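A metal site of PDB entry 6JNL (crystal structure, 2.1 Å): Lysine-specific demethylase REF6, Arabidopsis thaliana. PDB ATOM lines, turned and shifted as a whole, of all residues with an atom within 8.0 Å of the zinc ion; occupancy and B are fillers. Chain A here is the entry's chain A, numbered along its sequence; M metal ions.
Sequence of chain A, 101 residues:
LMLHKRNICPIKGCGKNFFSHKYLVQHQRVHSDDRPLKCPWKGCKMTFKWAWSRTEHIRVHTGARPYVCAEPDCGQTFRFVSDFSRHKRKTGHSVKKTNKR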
ATOM      1  N   VAL A  68     -14.857 -18.873 -21.240  1.00  0.00           N
ATOM      2  CA  VAL A  68     -13.876 -17.752 -21.269  1.00  0.00           C
ATOM      3  C   VAL A  68     -14.031 -17.020 -22.576  1.00  0.00           C
ATOM      4  O   VAL A  68     -13.755 -17.592 -23.614  1.00  0.00           O
ATOM      5  CB  VAL A  68     -12.429 -18.277 -21.128  1.00  0.00           C
ATOM      6  CG1 VAL A  68     -11.421 -17.137 -21.291  1.00  0.00           C
ATOM      7  CG2 VAL A  68     -12.264 -18.951 -19.749  1.00  0.00           C
ATOM      8  N   CYS A  69     -14.501 -15.766 -22.544  1.00  0.00           N
ATOM      9  CA  CYS A  69     -14.559 -14.935 -23.757  1.00  0.00           C
ATOM     10  C   CYS A  69     -13.197 -14.741 -24.418  1.00  0.00           C
ATOM     11  O   CYS A  69     -12.241 -14.339 -23.757  1.00  0.00           O
ATOM     12  CB  CYS A  69     -15.079 -13.561 -23.453  1.00  0.00           C
ATOM     13  SG  CYS A  69     -15.428 -12.827 -25.027  1.00  0.00           S
ATOM     14  N   ALA A  70     -13.102 -15.066 -25.714  1.00  0.00           N
ATOM     15  CA  ALA A  70     -11.863 -14.953 -26.506  1.00  0.00           C
ATOM     16  C   ALA A  70     -11.604 -13.544 -27.129  1.00  0.00           C
ATOM     17  O   ALA A  70     -10.496 -13.321 -27.545  1.00  0.00           O
ATOM     18  CB  ALA A  70     -11.861 -15.999 -27.600  1.00  0.00           C
ATOM     19  N   GLU A  71     -12.592 -12.637 -27.193  1.00  0.00           N
ATOM     20  CA  GLU A  71     -12.394 -11.278 -27.770  1.00  0.00           C
ATOM     21  C   GLU A  71     -11.145 -10.677 -27.189  1.00  0.00           C
ATOM     22  O   GLU A  71     -10.917 -10.800 -25.964  1.00  0.00           O
ATOM     23  CB  GLU A  71     -13.577 -10.323 -27.530  1.00  0.00           C
ATOM     24  CG  GLU A  71     -13.484  -8.963 -28.255  1.00  0.00           C
ATOM     25  CD  GLU A  71     -13.825  -9.007 -29.749  1.00  0.00           C
ATOM     26  OE1 GLU A  71     -14.230 -10.070 -30.256  1.00  0.00           O
ATOM     27  OE2 GLU A  71     -13.682  -7.954 -30.416  1.00  0.00           O
ATOM     28  N   PRO A  72     -10.308 -10.048 -28.069  1.00  0.00           N
ATOM     29  CA  PRO A  72      -9.063  -9.497 -27.537  1.00  0.00           C
ATOM     30  C   PRO A  72      -9.352  -8.503 -26.385  1.00  0.00           C
ATOM     31  O   PRO A  72     -10.219  -7.596 -26.563  1.00  0.00           O
ATOM     32  CB  PRO A  72      -8.425  -8.842 -28.789  1.00  0.00           C
ATOM     33  CG  PRO A  72      -8.950  -9.613 -29.960  1.00  0.00           C
ATOM     34  CD  PRO A  72     -10.370  -9.938 -29.549  1.00  0.00           C
ATOM     35  N   ASP A  73      -8.732  -8.725 -25.214  1.00  0.00           N
ATOM     36  CA  ASP A  73      -8.874  -7.787 -24.092  1.00  0.00           C
ATOM     37  C   ASP A  73     -10.254  -7.804 -23.375  1.00  0.00           C
ATOM     38  O   ASP A  73     -10.417  -7.036 -22.415  1.00  0.00           O
ATOM     39  CB  ASP A  73      -8.624  -6.286 -24.518  1.00  0.00           C
ATOM     40  CG  ASP A  73      -7.266  -6.054 -25.197  1.00  0.00           C
ATOM     41  OD1 ASP A  73      -6.253  -6.434 -24.597  1.00  0.00           O
ATOM     42  OD2 ASP A  73      -7.226  -5.435 -26.310  1.00  0.00           O
ATOM     43  N   CYS A  74     -11.228  -8.639 -23.805  1.00  0.00           N
ATOM     44  CA  CYS A  74     -12.523  -8.774 -23.064  1.00  0.00           C
ATOM     45  C   CYS A  74     -12.347  -9.277 -21.620  1.00  0.00           C
ATOM     46  O   CYS A  74     -12.924  -8.701 -20.695  1.00  0.00           O
ATOM     47  CB  CYS A  74     -13.569  -9.662 -23.767  1.00  0.00           C
ATOM     48  SG  CYS A  74     -15.054  -9.932 -22.753  1.00  0.00           S
ATOM     49  N   GLY A  75     -11.592 -10.362 -21.439  1.00  0.00           N
ATOM     50  CA  GLY A  75     -11.308 -10.915 -20.109  1.00  0.00           C
ATOM     51  C   GLY A  75     -12.495 -11.549 -19.311  1.00  0.00           C
ATOM     52  O   GLY A  75     -12.287 -12.033 -18.176  1.00  0.00           O
ATOM     53  N   GLN A  76     -13.712 -11.565 -19.858  1.00  0.00           N
ATOM     54  CA  GLN A  76     -14.832 -12.075 -19.072  1.00  0.00           C
ATOM     55  C   GLN A  76     -14.994 -13.603 -19.053  1.00  0.00           C
ATOM     56  O   GLN A  76     -14.661 -14.291 -20.030  1.00  0.00           O
ATOM     57  CB  GLN A  76     -16.088 -11.488 -19.569  1.00  0.00           C
ATOM     58  CG  GLN A  76     -16.196 -10.070 -19.095  1.00  0.00           C
ATOM     59  CD  GLN A  76     -17.520  -9.537 -19.453  1.00  0.00           C
ATOM     60  OE1 GLN A  76     -17.623  -8.575 -20.152  1.00  0.00           O
ATOM     61  NE2 GLN A  76     -18.573 -10.205 -19.005  1.00  0.00           N
ATOM     62  N   THR A  77     -15.476 -14.115 -17.930  1.00  0.00           N
ATOM     63  CA  THR A  77     -15.662 -15.559 -17.791  1.00  0.00           C
ATOM     64  C   THR A  77     -17.028 -15.870 -17.226  1.00  0.00           C
ATOM     65  O   THR A  77     -17.642 -15.018 -16.617  1.00  0.00           O
ATOM     66  CB  THR A  77     -14.569 -16.220 -16.966  1.00  0.00           C
ATOM     67  OG1 THR A  77     -14.774 -15.911 -15.589  1.00  0.00           O
ATOM     68  CG2 THR A  77     -13.240 -15.750 -17.413  1.00  0.00           C
ATOM     69  N   PHE A  78     -17.530 -17.071 -17.493  1.00  0.00           N
ATOM     70  CA  PHE A  78     -18.891 -17.440 -17.077  1.00  0.00           C
ATOM     71  C   PHE A  78     -18.988 -18.855 -16.497  1.00  0.00           C
ATOM     72  O   PHE A  78     -18.248 -19.782 -16.890  1.00  0.00           O
ATOM     73  CB  PHE A  78     -19.843 -17.267 -18.226  1.00  0.00           C
ATOM     74  CG  PHE A  78     -19.745 -15.929 -18.844  1.00  0.00           C
ATOM     75  CD1 PHE A  78     -18.778 -15.687 -19.801  1.00  0.00           C
ATOM     76  CD2 PHE A  78     -20.548 -14.892 -18.396  1.00  0.00           C
ATOM     77  CE1 PHE A  78     -18.643 -14.410 -20.353  1.00  0.00           C
ATOM     78  CE2 PHE A  78     -20.452 -13.639 -18.950  1.00  0.00           C
ATOM     79  CZ  PHE A  78     -19.476 -13.389 -19.919  1.00  0.00           C
ATOM     80  N   PHE A  84     -22.797 -17.098 -21.168  1.00  0.00           N
ATOM     81  CA  PHE A  84     -21.773 -16.908 -22.156  1.00  0.00           C
ATOM     82  C   PHE A  84     -22.345 -16.592 -23.549  1.00  0.00           C
ATOM     83  O   PHE A  84     -21.865 -15.667 -24.231  1.00  0.00           O
ATOM     84  CB  PHE A  84     -20.865 -18.075 -22.155  1.00  0.00           C
ATOM     85  CG  PHE A  84     -19.739 -17.986 -23.145  1.00  0.00           C
ATOM     86  CD1 PHE A  84     -19.004 -16.819 -23.334  1.00  0.00           C
ATOM     87  CD2 PHE A  84     -19.357 -19.146 -23.878  1.00  0.00           C
ATOM     88  CE1 PHE A  84     -17.949 -16.777 -24.260  1.00  0.00           C
ATOM     89  CE2 PHE A  84     -18.275 -19.122 -24.765  1.00  0.00           C
ATOM     90  CZ  PHE A  84     -17.575 -17.922 -24.973  1.00  0.00           C
ATOM     91  N   HIS A  87     -23.857 -13.005 -23.555  1.00  0.00           N
ATOM     92  CA  HIS A  87     -22.799 -12.008 -23.709  1.00  0.00           C
ATOM     93  C   HIS A  87     -22.230 -11.862 -25.136  1.00  0.00           C
ATOM     94  O   HIS A  87     -21.961 -10.770 -25.594  1.00  0.00           O
ATOM     95  CB  HIS A  87     -21.711 -12.278 -22.715  1.00  0.00           C
ATOM     96  CG  HIS A  87     -20.378 -11.670 -23.059  1.00  0.00           C
ATOM     97  ND1 HIS A  87     -20.080 -10.340 -22.850  1.00  0.00           N
ATOM     98  CD2 HIS A  87     -19.237 -12.242 -23.506  1.00  0.00           C
ATOM     99  CE1 HIS A  87     -18.826 -10.114 -23.160  1.00  0.00           C
ATOM    100  NE2 HIS A  87     -18.297 -11.255 -23.574  1.00  0.00           N
ATOM    101  N   LYS A  88     -22.046 -12.949 -25.832  1.00  0.00           N
ATOM    102  CA  LYS A  88     -21.693 -12.893 -27.224  1.00  0.00           C
ATOM    103  C   LYS A  88     -22.772 -12.201 -28.091  1.00  0.00           C
ATOM    104  O   LYS A  88     -22.473 -11.392 -28.948  1.00  0.00           O
ATOM    105  CB  LYS A  88     -21.550 -14.316 -27.739  1.00  0.00           C
ATOM    106  CG  LYS A  88     -20.382 -15.099 -27.186  1.00  0.00           C
ATOM    107  CD  LYS A  88     -20.708 -16.579 -27.341  1.00  0.00           C
ATOM    108  CE  LYS A  88     -19.519 -17.408 -27.771  1.00  0.00           C
ATOM    109  NZ  LYS A  88     -20.009 -18.796 -27.933  1.00  0.00           N
ATOM    110  N   THR A  91     -22.769  -8.495 -27.204  1.00  0.00           N
ATOM    111  CA  THR A  91     -21.559  -7.783 -27.560  1.00  0.00           C
ATOM    112  C   THR A  91     -20.930  -8.018 -28.937  1.00  0.00           C
ATOM    113  O   THR A  91     -20.131  -7.222 -29.361  1.00  0.00           O
ATOM    114  CB  THR A  91     -20.432  -8.089 -26.538  1.00  0.00           C
ATOM    115  OG1 THR A  91     -19.944  -9.447 -26.683  1.00  0.00           O
ATOM    116  CG2 THR A  91     -20.925  -7.806 -25.128  1.00  0.00           C
ATOM    117  N   GLY A  92     -21.231  -9.139 -29.580  1.00  0.00           N
ATOM    118  CA  GLY A  92     -20.546  -9.518 -30.835  1.00  0.00           C
ATOM    119  C   GLY A  92     -19.217 -10.259 -30.770  1.00  0.00           C
ATOM    120  O   GLY A  92     -18.589 -10.487 -31.809  1.00  0.00           O
ATOM    121  N   HIS A  93     -18.790 -10.685 -29.579  1.00  0.00           N
ATOM    122  CA  HIS A  93     -17.502 -11.412 -29.409  1.00  0.00           C
ATOM    123  C   HIS A  93     -17.713 -12.857 -29.917  1.00  0.00           C
ATOM    124  O   HIS A  93     -18.797 -13.384 -29.730  1.00  0.00           O
ATOM    125  CB  HIS A  93     -17.089 -11.336 -27.948  1.00  0.00           C
ATOM    126  CG  HIS A  93     -17.005  -9.936 -27.420  1.00  0.00           C
ATOM    127  ND1 HIS A  93     -16.295  -9.609 -26.278  1.00  0.00           N
ATOM    128  CD2 HIS A  93     -17.496  -8.768 -27.880  1.00  0.00           C
ATOM    129  CE1 HIS A  93     -16.376  -8.311 -26.053  1.00  0.00           C
ATOM    130  NE2 HIS A  93     -17.106  -7.782 -27.012  1.00  0.00           N
ATOM    131  N   SER A  94     -16.736 -13.467 -30.612  1.00  0.00           N
ATOM    132  CA  SER A  94     -16.920 -14.678 -31.504  1.00  0.00           C
ATOM    133  C   SER A  94     -18.191 -14.683 -32.368  1.00  0.00           C
ATOM    134  O   SER A  94     -18.255 -15.416 -33.348  1.00  0.00           O
ATOM    135  CB  SER A  94     -16.840 -16.001 -30.720  1.00  0.00           C
ATOM    136  OG  SER A  94     -15.983 -15.869 -29.597  1.00  0.00           O
HETATM  137 ZN    ZN M   1     -16.362 -10.822 -24.454  1.00  0.00          ZN
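The side-chain hydroxyl (OG1) of Thr 91 lies within hydrogen-bond range of the backbone carbonyl oxygen (O) of His 87 (2.6 Å). NE2 of His 93 sits close to OG1 of Thr 91, 3.3 Å away. SG of Cys 69 lies close to N of Glu 71, at 3.6 Å. The backbone NH (N) of Cys 69 sits at hydrogen-bond distance from the backbone carbonyl oxygen (O) of Gln 76 (2.9 Å). The backbone NH of Gln 76 sits close to the side-chain sulfur of Cys 74.
The zinc ion is bound by a ring nitrogen (NE2) of His 87 (2.2 Å), a ring nitrogen (ND1) of His 93 (2.2 Å), the side-chain sulfur (SG) of Cys 69 (2.3 Å) and the side-chain sulfur (SG) of Cys 74 (2.3 Å). The zinc ion has four donor atoms within binding distance.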
